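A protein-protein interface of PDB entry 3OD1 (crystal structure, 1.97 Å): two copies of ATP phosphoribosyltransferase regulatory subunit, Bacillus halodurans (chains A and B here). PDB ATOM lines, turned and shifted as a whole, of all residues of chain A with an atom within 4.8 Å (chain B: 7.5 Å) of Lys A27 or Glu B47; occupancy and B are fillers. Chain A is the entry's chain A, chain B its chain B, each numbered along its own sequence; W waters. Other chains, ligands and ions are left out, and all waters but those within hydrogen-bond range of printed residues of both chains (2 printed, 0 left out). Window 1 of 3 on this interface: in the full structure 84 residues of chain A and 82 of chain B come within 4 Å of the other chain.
OD1 of Asp B44 is in salt-bridge range of NZ of Lys A25. The guanidinium group (NH1) of Arg B91 is in salt-bridge range of the side-chain carboxylate (OD2) of Asp A18 (2.8 Å). NZ of Lys A27 is in salt-bridge range of OE2 of Glu B47. The backbone NH (N) of Thr A19 sits at hydrogen-bond distance from the backbone carbonyl oxygen (O) of Glu B47, at 2.8 Å.
Position printed for both chains: 109. Of the 11 pairs that touch across the chains among the printed residues, none has its exchanged pair printed and touching as well.
Water W1 lies within hydrogen-bond range of OH of Tyr A24, OE2 of Glu B47 and O of Gln B109. Water W2 lies within hydrogen-bond range of NZ of Lys A27 (2.8 Å), OE2 of Glu A127 (2.9 Å), NE2 of Gln A109 (3.4 Å) and OE2 of Glu B47 (3.5 Å).
C of Asp A18 touches O of Glu B47, 3.7 Å away. Asp A18 touches Thr B48 (OD1 to CA, 3.7 Å). Asp A18 touches Pro B49. Asp A18 touches Leu B92. O of Thr A19 touches CB of Ile B46, at 3.4 Å. OH of Tyr A24 touches CE of Met B45 (3.0 Å). Glu B47 touches Tyr A24.
NH1 of Arg B82 is in hydrogen-bond range of O of Thr B48 (2.9 Å). O of Asp B44 sits at hydrogen-bond distance from N of Ala B107 (2.9 Å). O of Ala B107 lies within hydrogen-bond range of N of Ile B46 (3.0 Å). O of Lys A27 is in hydrogen-bond range of SG of Cys A31 (3.5 Å). O of Pro B49 lies within hydrogen-bond range of NH1 of Arg B82 (2.9 Å). The side-chain sulfur (SD) of Met B85 sits close to the side-chain hydroxyl (OG1) of Thr B48 (3.1 Å).
Hydrophobic or aromatic side chains of chain B within 4 Å of the printed part of chain A: Met B45, Ile B46, Pro B49 and Leu B92. Of the 15 printed residues of chain A, 5 touch a printed residue of chain B. Along chain A the printed residues that touch a printed residue of chain B span positions 18 to 27.
Of chain A, only Asp A18, Thr A19, Tyr A24 and Lys A27 come within 4 Å of Glu B47. Printed residues of chain B within 4 Å of Thr A19: Ile B46 (3.4 Å) and Glu B47 (2.8 Å). Of the printed residues of chain A, Arg B91 touches Asp A18. Lys A28 touches none of the printed residues of chain B. The nearest residue of chain A that does not touch Glu B47 is Glu A127 (4.6 Å). The nearest printed residue of chain A that does not touch Met B45 is Thr A19 (4.9 Å).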
ATOM      1  N   ASP A  18     -23.044 -27.122 -12.098  1.00  0.00           N
ATOM      2  CA  ASP A  18     -22.905 -25.715 -11.697  1.00  0.00           C
ATOM      3  C   ASP A  18     -24.281 -25.058 -11.540  1.00  0.00           C
ATOM      4  O   ASP A  18     -25.246 -25.482 -12.166  1.00  0.00           O
ATOM      5  CB  ASP A  18     -22.093 -24.909 -12.733  1.00  0.00           C
ATOM      6  CG  ASP A  18     -20.606 -25.227 -12.704  1.00  0.00           C
ATOM      7  OD1 ASP A  18     -20.061 -25.482 -11.611  1.00  0.00           O
ATOM      8  OD2 ASP A  18     -19.973 -25.210 -13.786  1.00  0.00           O
ATOM      9  N   THR A  19     -24.358 -24.009 -10.727  1.00  0.00           N
ATOM     10  CA  THR A  19     -25.580 -23.213 -10.614  1.00  0.00           C
ATOM     11  C   THR A  19     -25.322 -21.768 -11.089  1.00  0.00           C
ATOM     12  O   THR A  19     -24.687 -20.970 -10.396  1.00  0.00           O
ATOM     13  CB  THR A  19     -26.147 -23.240  -9.167  1.00  0.00           C
ATOM     14  OG1 THR A  19     -26.400 -24.596  -8.776  1.00  0.00           O
ATOM     15  CG2 THR A  19     -27.450 -22.427  -9.062  1.00  0.00           C
ATOM     16  N   TRP A  23     -30.408 -19.006 -12.453  1.00  0.00           N
ATOM     17  CA  TRP A  23     -30.962 -20.173 -11.789  1.00  0.00           C
ATOM     18  C   TRP A  23     -30.752 -20.035 -10.282  1.00  0.00           C
ATOM     19  O   TRP A  23     -31.610 -20.434  -9.494  1.00  0.00           O
ATOM     20  CB  TRP A  23     -30.284 -21.442 -12.304  1.00  0.00           C
ATOM     21  CG  TRP A  23     -31.085 -22.700 -12.094  1.00  0.00           C
ATOM     22  CD1 TRP A  23     -31.909 -23.306 -13.003  1.00  0.00           C
ATOM     23  CD2 TRP A  23     -31.137 -23.510 -10.904  1.00  0.00           C
ATOM     24  NE1 TRP A  23     -32.465 -24.439 -12.456  1.00  0.00           N
ATOM     25  CE2 TRP A  23     -32.007 -24.588 -11.170  1.00  0.00           C
ATOM     26  CE3 TRP A  23     -30.531 -23.427  -9.644  1.00  0.00           C
ATOM     27  CZ2 TRP A  23     -32.291 -25.579 -10.221  1.00  0.00           C
ATOM     28  CZ3 TRP A  23     -30.808 -24.418  -8.699  1.00  0.00           C
ATOM     29  CH2 TRP A  23     -31.685 -25.475  -8.993  1.00  0.00           C
ATOM     30  N   TYR A  24     -29.619 -19.460  -9.886  1.00  0.00           N
ATOM     31  CA  TYR A  24     -29.349 -19.247  -8.473  1.00  0.00           C
ATOM     32  C   TYR A  24     -30.375 -18.310  -7.846  1.00  0.00           C
ATOM     33  O   TYR A  24     -30.882 -18.601  -6.771  1.00  0.00           O
ATOM     34  CB  TYR A  24     -27.948 -18.696  -8.205  1.00  0.00           C
ATOM     35  CG  TYR A  24     -27.689 -18.537  -6.718  1.00  0.00           C
ATOM     36  CD1 TYR A  24     -27.073 -19.547  -5.993  1.00  0.00           C
ATOM     37  CD2 TYR A  24     -28.108 -17.402  -6.031  1.00  0.00           C
ATOM     38  CE1 TYR A  24     -26.861 -19.423  -4.638  1.00  0.00           C
ATOM     39  CE2 TYR A  24     -27.898 -17.273  -4.670  1.00  0.00           C
ATOM     40  CZ  TYR A  24     -27.271 -18.287  -3.984  1.00  0.00           C
ATOM     41  OH  TYR A  24     -27.052 -18.173  -2.628  1.00  0.00           O
ATOM     42  N   LYS A  25     -30.667 -17.189  -8.500  1.00  0.00           N
ATOM     43  CA  LYS A  25     -31.664 -16.262  -7.969  1.00  0.00           C
ATOM     44  C   LYS A  25     -33.044 -16.919  -7.855  1.00  0.00           C
ATOM     45  O   LYS A  25     -33.743 -16.746  -6.853  1.00  0.00           O
ATOM     46  CB  LYS A  25     -31.759 -14.989  -8.811  1.00  0.00           C
ATOM     47  CG  LYS A  25     -30.525 -14.102  -8.731  1.00  0.00           C
ATOM     48  CD  LYS A  25     -30.779 -12.737  -9.367  1.00  0.00           C
ATOM     49  CE  LYS A  25     -29.473 -12.057  -9.791  1.00  0.00           C
ATOM     50  NZ  LYS A  25     -28.974 -12.550 -11.114  1.00  0.00           N
ATOM     51  N   THR A  26     -33.431 -17.660  -8.882  1.00  0.00           N
ATOM     52  CA  THR A  26     -34.712 -18.375  -8.858  1.00  0.00           C
ATOM     53  C   THR A  26     -34.774 -19.341  -7.664  1.00  0.00           C
ATOM     54  O   THR A  26     -35.727 -19.317  -6.886  1.00  0.00           O
ATOM     55  CB  THR A  26     -34.969 -19.139 -10.171  1.00  0.00           C
ATOM     56  OG1 THR A  26     -34.946 -18.221 -11.270  1.00  0.00           O
ATOM     57  CG2 THR A  26     -36.334 -19.808 -10.136  1.00  0.00           C
ATOM     58  N   LYS A  27     -33.745 -20.168  -7.512  1.00  0.00           N
ATOM     59  CA  LYS A  27     -33.681 -21.133  -6.427  1.00  0.00           C
ATOM     60  C   LYS A  27     -33.645 -20.434  -5.066  1.00  0.00           C
ATOM     61  O   LYS A  27     -34.370 -20.814  -4.153  1.00  0.00           O
ATOM     62  CB  LYS A  27     -32.486 -22.086  -6.625  1.00  0.00           C
ATOM     63  CG  LYS A  27     -31.899 -22.715  -5.363  1.00  0.00           C
ATOM     64  CD  LYS A  27     -30.839 -21.827  -4.695  1.00  0.00           C
ATOM     65  CE  LYS A  27     -29.643 -22.655  -4.208  1.00  0.00           C
ATOM     66  NZ  LYS A  27     -29.136 -22.260  -2.843  1.00  0.00           N
ATOM     67  N   LYS A  28     -32.832 -19.391  -4.933  1.00  0.00           N
ATOM     68  CA  LYS A  28     -32.762 -18.675  -3.663  1.00  0.00           C
ATOM     69  C   LYS A  28     -34.123 -18.114  -3.220  1.00  0.00           C
ATOM     70  O   LYS A  28     -34.495 -18.229  -2.052  1.00  0.00           O
ATOM     71  CB  LYS A  28     -31.720 -17.559  -3.709  1.00  0.00           C
ATOM     72  CG  LYS A  28     -31.759 -16.645  -2.500  1.00  0.00           C
ATOM     73  CD  LYS A  28     -30.617 -15.643  -2.515  1.00  0.00           C
ATOM     74  CE  LYS A  28     -30.803 -14.630  -1.404  1.00  0.00           C
ATOM     75  NZ  LYS A  28     -30.902 -15.297  -0.075  1.00  0.00           N
ATOM     76  N   ASN A  29     -34.855 -17.489  -4.133  1.00  0.00           N
ATOM     77  CA  ASN A  29     -36.169 -16.948  -3.774  1.00  0.00           C
ATOM     78  C   ASN A  29     -37.154 -18.029  -3.328  1.00  0.00           C
ATOM     79  O   ASN A  29     -37.879 -17.866  -2.343  1.00  0.00           O
ATOM     80  CB  ASN A  29     -36.782 -16.162  -4.929  1.00  0.00           C
ATOM     81  CG  ASN A  29     -38.235 -15.760  -4.649  1.00  0.00           C
ATOM     82  OD1 ASN A  29     -38.536 -15.147  -3.620  1.00  0.00           O
ATOM     83  ND2 ASN A  29     -39.138 -16.117  -5.560  1.00  0.00           N
ATOM     84  N   ILE A  30     -37.197 -19.116  -4.083  1.00  0.00           N
ATOM     85  CA  ILE A  30     -38.023 -20.258  -3.730  1.00  0.00           C
ATOM     86  C   ILE A  30     -37.695 -20.755  -2.328  1.00  0.00           C
ATOM     87  O   ILE A  30     -38.587 -20.857  -1.491  1.00  0.00           O
ATOM     88  CB  ILE A  30     -37.875 -21.387  -4.771  1.00  0.00           C
ATOM     89  CG1 ILE A  30     -38.646 -21.017  -6.042  1.00  0.00           C
ATOM     90  CG2 ILE A  30     -38.353 -22.718  -4.208  1.00  0.00           C
ATOM     91  CD1 ILE A  30     -38.245 -21.811  -7.261  1.00  0.00           C
ATOM     92  N   CYS A  31     -36.420 -21.034  -2.057  1.00  0.00           N
ATOM     93  CA  CYS A  31     -36.022 -21.556  -0.743  1.00  0.00           C
ATOM     94  C   CYS A  31     -36.273 -20.560   0.392  1.00  0.00           C
ATOM     95  O   CYS A  31     -36.652 -20.959   1.496  1.00  0.00           O
ATOM     96  CB  CYS A  31     -34.550 -21.997  -0.733  1.00  0.00           C
ATOM     97  SG  CYS A  31     -34.141 -23.377  -1.840  1.00  0.00           S
ATOM     98  N   GLN A 109     -31.585 -26.771   5.203  1.00  0.00           N
ATOM     99  CA  GLN A 109     -31.560 -26.565   3.768  1.00  0.00           C
ATOM    100  C   GLN A 109     -30.140 -26.918   3.411  1.00  0.00           C
ATOM    101  O   GLN A 109     -29.220 -26.152   3.701  1.00  0.00           O
ATOM    102  CB  GLN A 109     -31.860 -25.107   3.431  1.00  0.00           C
ATOM    103  CG  GLN A 109     -31.754 -24.802   1.933  1.00  0.00           C
ATOM    104  CD  GLN A 109     -31.889 -23.310   1.621  1.00  0.00           C
ATOM    105  OE1 GLN A 109     -32.478 -22.554   2.390  1.00  0.00           O
ATOM    106  NE2 GLN A 109     -31.345 -22.888   0.476  1.00  0.00           N
ATOM    107  N   GLU A 127     -29.957 -30.043  -3.683  1.00  0.00           N
ATOM    108  CA  GLU A 127     -30.343 -29.336  -2.474  1.00  0.00           C
ATOM    109  C   GLU A 127     -31.667 -29.859  -1.942  1.00  0.00           C
ATOM    110  O   GLU A 127     -32.602 -30.091  -2.706  1.00  0.00           O
ATOM    111  CB  GLU A 127     -30.443 -27.840  -2.767  1.00  0.00           C
ATOM    112  CG  GLU A 127     -30.563 -26.988  -1.524  1.00  0.00           C
ATOM    113  CD  GLU A 127     -30.208 -25.542  -1.789  1.00  0.00           C
ATOM    114  OE1 GLU A 127     -30.337 -25.112  -2.957  1.00  0.00           O
ATOM    115  OE2 GLU A 127     -29.800 -24.847  -0.832  1.00  0.00           O
ATOM    116  N   ILE A 320     -35.321 -29.561  -3.886  1.00  0.00           N
ATOM    117  CA  ILE A 320     -35.305 -28.227  -4.467  1.00  0.00           C
ATOM    118  C   ILE A 320     -35.153 -28.223  -5.983  1.00  0.00           C
ATOM    119  O   ILE A 320     -35.857 -27.483  -6.667  1.00  0.00           O
ATOM    120  CB  ILE A 320     -34.228 -27.348  -3.803  1.00  0.00           C
ATOM    121  CG1 ILE A 320     -34.580 -27.153  -2.325  1.00  0.00           C
ATOM    122  CG2 ILE A 320     -34.113 -25.989  -4.492  1.00  0.00           C
ATOM    123  CD1 ILE A 320     -36.012 -26.628  -2.118  1.00  0.00           C
ATOM    124  N   VAL A 324     -37.908 -26.526  -8.354  1.00  0.00           N
ATOM    125  CA  VAL A 324     -37.596 -25.477  -9.320  1.00  0.00           C
ATOM    126  C   VAL A 324     -38.087 -25.877 -10.709  1.00  0.00           C
ATOM    127  O   VAL A 324     -38.725 -25.094 -11.416  1.00  0.00           O
ATOM    128  CB  VAL A 324     -36.073 -25.207  -9.384  1.00  0.00           C
ATOM    129  CG1 VAL A 324     -35.731 -24.382 -10.616  1.00  0.00           C
ATOM    130  CG2 VAL A 324     -35.593 -24.517  -8.109  1.00  0.00           C
ATOM    131  N   ASP B  44     -23.169 -11.222  -8.811  1.00  0.00           N
ATOM    132  CA  ASP B  44     -24.192 -12.277  -8.883  1.00  0.00           C
ATOM    133  C   ASP B  44     -23.686 -13.522  -8.171  1.00  0.00           C
ATOM    134  O   ASP B  44     -22.616 -14.046  -8.503  1.00  0.00           O
ATOM    135  CB  ASP B  44     -24.495 -12.680 -10.327  1.00  0.00           C
ATOM    136  CG  ASP B  44     -25.186 -11.587 -11.127  1.00  0.00           C
ATOM    137  OD1 ASP B  44     -26.079 -10.894 -10.605  1.00  0.00           O
ATOM    138  OD2 ASP B  44     -24.852 -11.456 -12.307  1.00  0.00           O
ATOM    139  N   MET B  45     -24.460 -14.001  -7.206  1.00  0.00           N
ATOM    140  CA  MET B  45     -24.167 -15.273  -6.541  1.00  0.00           C
ATOM    141  C   MET B  45     -24.247 -16.449  -7.502  1.00  0.00           C
ATOM    142  O   MET B  45     -25.137 -16.512  -8.351  1.00  0.00           O
ATOM    143  CB  MET B  45     -25.154 -15.477  -5.383  1.00  0.00           C
ATOM    144  CG  MET B  45     -25.032 -14.392  -4.346  1.00  0.00           C
ATOM    145  SD  MET B  45     -23.661 -14.895  -3.073  1.00  0.00           S
ATOM    146  CE  MET B  45     -24.661 -16.437  -2.395  1.00  0.00           C
ATOM    147  N   ILE B  46     -23.309 -17.383  -7.375  1.00  0.00           N
ATOM    148  CA  ILE B  46     -23.399 -18.652  -8.083  1.00  0.00           C
ATOM    149  C   ILE B  46     -23.153 -19.792  -7.107  1.00  0.00           C
ATOM    150  O   ILE B  46     -22.844 -19.548  -5.927  1.00  0.00           O
ATOM    151  CB  ILE B  46     -22.410 -18.739  -9.282  1.00  0.00           C
ATOM    152  CG1 ILE B  46     -21.010 -18.259  -8.884  1.00  0.00           C
ATOM    153  CG2 ILE B  46     -22.946 -17.940 -10.463  1.00  0.00           C
ATOM    154  CD1 ILE B  46     -20.227 -19.274  -8.029  1.00  0.00           C
ATOM    155  N   GLU B  47     -23.327 -21.025  -7.581  1.00  0.00           N
ATOM    156  CA  GLU B  47     -22.824 -22.184  -6.849  1.00  0.00           C
ATOM    157  C   GLU B  47     -22.096 -23.138  -7.784  1.00  0.00           C
ATOM    158  O   GLU B  47     -22.364 -23.181  -8.986  1.00  0.00           O
ATOM    159  CB  GLU B  47     -23.938 -22.904  -6.077  1.00  0.00           C
ATOM    160  CG  GLU B  47     -24.556 -22.012  -5.000  1.00  0.00           C
ATOM    161  CD  GLU B  47     -25.725 -22.657  -4.240  1.00  0.00           C
ATOM    162  OE1 GLU B  47     -26.398 -23.555  -4.794  1.00  0.00           O
ATOM    163  OE2 GLU B  47     -25.971 -22.241  -3.082  1.00  0.00           O
ATOM    164  N   THR B  48     -21.142 -23.873  -7.229  1.00  0.00           N
ATOM    165  CA  THR B  48     -20.400 -24.882  -7.982  1.00  0.00           C
ATOM    166  C   THR B  48     -20.490 -26.172  -7.174  1.00  0.00           C
ATOM    167  O   THR B  48     -20.984 -26.152  -6.037  1.00  0.00           O
ATOM    168  CB  THR B  48     -18.924 -24.479  -8.144  1.00  0.00           C
ATOM    169  OG1 THR B  48     -18.356 -24.283  -6.844  1.00  0.00           O
ATOM    170  CG2 THR B  48     -18.792 -23.193  -8.957  1.00  0.00           C
ATOM    171  N   PRO B  49     -20.025 -27.299  -7.741  1.00  0.00           N
ATOM    172  CA  PRO B  49     -20.234 -28.588  -7.064  1.00  0.00           C
ATOM    173  C   PRO B  49     -19.327 -28.776  -5.866  1.00  0.00           C
ATOM    174  O   PRO B  49     -18.293 -28.115  -5.731  1.00  0.00           O
ATOM    175  CB  PRO B  49     -19.849 -29.625  -8.132  1.00  0.00           C
ATOM    176  CG  PRO B  49     -19.905 -28.865  -9.442  1.00  0.00           C
ATOM    177  CD  PRO B  49     -19.452 -27.478  -9.089  1.00  0.00           C
ATOM    178  N   ARG B  82     -14.037 -29.390  -2.782  1.00  0.00           N
ATOM    179  CA  ARG B  82     -13.520 -28.095  -3.214  1.00  0.00           C
ATOM    180  C   ARG B  82     -12.748 -27.346  -2.125  1.00  0.00           C
ATOM    181  O   ARG B  82     -13.262 -27.076  -1.020  1.00  0.00           O
ATOM    182  CB  ARG B  82     -14.616 -27.217  -3.784  1.00  0.00           C
ATOM    183  CG  ARG B  82     -15.714 -26.991  -2.818  1.00  0.00           C
ATOM    184  CD  ARG B  82     -16.470 -25.743  -3.151  1.00  0.00           C
ATOM    185  NE  ARG B  82     -17.581 -25.580  -2.229  1.00  0.00           N
ATOM    186  CZ  ARG B  82     -18.841 -25.835  -2.536  1.00  0.00           C
ATOM    187  NH1 ARG B  82     -19.154 -26.239  -3.754  1.00  0.00           N
ATOM    188  NH2 ARG B  82     -19.788 -25.646  -1.634  1.00  0.00           N
ATOM    189  N   MET B  85     -13.360 -21.324  -3.748  1.00  0.00           N
ATOM    190  CA  MET B  85     -14.342 -20.988  -4.779  1.00  0.00           C
ATOM    191  C   MET B  85     -13.752 -20.268  -5.999  1.00  0.00           C
ATOM    192  O   MET B  85     -14.414 -20.151  -7.036  1.00  0.00           O
ATOM    193  CB  MET B  85     -15.505 -20.184  -4.184  1.00  0.00           C
ATOM    194  CG  MET B  85     -16.533 -21.067  -3.422  1.00  0.00           C
ATOM    195  SD  MET B  85     -17.291 -22.474  -4.560  1.00  0.00           S
ATOM    196  CE  MET B  85     -18.267 -21.366  -5.837  1.00  0.00           C
ATOM    197  N   PRO B  88     -12.927 -22.969  -8.871  1.00  0.00           N
ATOM    198  CA  PRO B  88     -14.197 -23.383  -9.480  1.00  0.00           C
ATOM    199  C   PRO B  88     -14.851 -22.243 -10.256  1.00  0.00           C
ATOM    200  O   PRO B  88     -15.397 -22.487 -11.326  1.00  0.00           O
ATOM    201  CB  PRO B  88     -15.046 -23.817  -8.273  1.00  0.00           C
ATOM    202  CG  PRO B  88     -14.007 -24.340  -7.293  1.00  0.00           C
ATOM    203  CD  PRO B  88     -12.830 -23.386  -7.456  1.00  0.00           C
ATOM    204  N   ILE B  89     -14.772 -21.013  -9.757  1.00  0.00           N
ATOM    205  CA  ILE B  89     -15.375 -19.910 -10.498  1.00  0.00           C
ATOM    206  C   ILE B  89     -14.617 -19.666 -11.816  1.00  0.00           C
ATOM    207  O   ILE B  89     -15.221 -19.361 -12.837  1.00  0.00           O
ATOM    208  CB  ILE B  89     -15.497 -18.636  -9.643  1.00  0.00           C
ATOM    209  CG1 ILE B  89     -16.666 -18.798  -8.660  1.00  0.00           C
ATOM    210  CG2 ILE B  89     -15.697 -17.410 -10.531  1.00  0.00           C
ATOM    211  CD1 ILE B  89     -16.759 -17.710  -7.630  1.00  0.00           C
ATOM    212  N   ARG B  91     -13.182 -21.972 -13.616  1.00  0.00           N
ATOM    213  CA  ARG B  91     -13.697 -23.020 -14.500  1.00  0.00           C
ATOM    214  C   ARG B  91     -15.049 -22.621 -15.082  1.00  0.00           C
ATOM    215  O   ARG B  91     -15.301 -22.773 -16.276  1.00  0.00           O
ATOM    216  CB  ARG B  91     -13.823 -24.375 -13.780  1.00  0.00           C
ATOM    217  CG  ARG B  91     -14.379 -25.504 -14.696  1.00  0.00           C
ATOM    218  CD  ARG B  91     -14.568 -26.849 -13.968  1.00  0.00           C
ATOM    219  NE  ARG B  91     -15.325 -26.711 -12.721  1.00  0.00           N
ATOM    220  CZ  ARG B  91     -16.570 -26.248 -12.632  1.00  0.00           C
ATOM    221  NH1 ARG B  91     -17.232 -25.882 -13.722  1.00  0.00           N
ATOM    222  NH2 ARG B  91     -17.155 -26.142 -11.440  1.00  0.00           N
ATOM    223  N   LEU B  92     -15.918 -22.111 -14.221  1.00  0.00           N
ATOM    224  CA  LEU B  92     -17.271 -21.745 -14.615  1.00  0.00           C
ATOM    225  C   LEU B  92     -17.202 -20.668 -15.682  1.00  0.00           C
ATOM    226  O   LEU B  92     -17.857 -20.763 -16.725  1.00  0.00           O
ATOM    227  CB  LEU B  92     -18.019 -21.233 -13.383  1.00  0.00           C
ATOM    228  CG  LEU B  92     -19.531 -21.367 -13.267  1.00  0.00           C
ATOM    229  CD1 LEU B  92     -19.986 -20.726 -11.977  1.00  0.00           C
ATOM    230  CD2 LEU B  92     -20.197 -20.702 -14.446  1.00  0.00           C
ATOM    231  N   ALA B 107     -20.119 -13.940  -7.022  1.00  0.00           N
ATOM    232  CA  ALA B 107     -20.041 -14.033  -5.565  1.00  0.00           C
ATOM    233  C   ALA B 107     -20.439 -15.425  -5.115  1.00  0.00           C
ATOM    234  O   ALA B 107     -21.046 -16.186  -5.877  1.00  0.00           O
ATOM    235  CB  ALA B 107     -20.968 -12.993  -4.877  1.00  0.00           C
ATOM    236  N   TYR B 108     -20.092 -15.771  -3.879  1.00  0.00           N
ATOM    237  CA  TYR B 108     -20.434 -17.091  -3.364  1.00  0.00           C
ATOM    238  C   TYR B 108     -20.557 -17.053  -1.853  1.00  0.00           C
ATOM    239  O   TYR B 108     -20.037 -16.156  -1.203  1.00  0.00           O
ATOM    240  CB  TYR B 108     -19.359 -18.108  -3.757  1.00  0.00           C
ATOM    241  CG  TYR B 108     -17.990 -17.728  -3.231  1.00  0.00           C
ATOM    242  CD1 TYR B 108     -17.150 -16.902  -3.966  1.00  0.00           C
ATOM    243  CD2 TYR B 108     -17.553 -18.166  -1.982  1.00  0.00           C
ATOM    244  CE1 TYR B 108     -15.884 -16.537  -3.486  1.00  0.00           C
ATOM    245  CE2 TYR B 108     -16.295 -17.803  -1.486  1.00  0.00           C
ATOM    246  CZ  TYR B 108     -15.462 -16.994  -2.245  1.00  0.00           C
ATOM    247  OH  TYR B 108     -14.219 -16.627  -1.750  1.00  0.00           O
ATOM    248  N   GLN B 109     -21.272 -18.032  -1.308  1.00  0.00           N
ATOM    249  CA  GLN B 109     -21.254 -18.306   0.114  1.00  0.00           C
ATOM    250  C   GLN B 109     -21.286 -19.831   0.187  1.00  0.00           C
ATOM    251  O   GLN B 109     -22.303 -20.460  -0.117  1.00  0.00           O
ATOM    252  CB  GLN B 109     -22.474 -17.686   0.799  1.00  0.00           C
ATOM    253  CG  GLN B 109     -22.540 -17.938   2.283  1.00  0.00           C
ATOM    254  CD  GLN B 109     -23.799 -17.354   2.925  1.00  0.00           C
ATOM    255  OE1 GLN B 109     -24.377 -16.391   2.417  1.00  0.00           O
ATOM    256  NE2 GLN B 109     -24.213 -17.929   4.060  1.00  0.00           N
ATOM    257  N   SER B 110     -20.158 -20.429   0.546  1.00  0.00           N
ATOM    258  CA  SER B 110     -19.995 -21.863   0.365  1.00  0.00           C
ATOM    259  C   SER B 110     -19.083 -22.480   1.401  1.00  0.00           C
ATOM    260  O   SER B 110     -18.130 -21.848   1.871  1.00  0.00           O
ATOM    261  CB  SER B 110     -19.391 -22.154  -1.016  1.00  0.00           C
ATOM    262  OG  SER B 110     -20.152 -21.573  -2.056  1.00  0.00           O
HETATM  263  O   HOH W   1     -25.264 -19.919  -1.571  1.00  0.00           O
HETATM  264  O   HOH W   2     -28.078 -22.625  -0.324  1.00  0.00           O
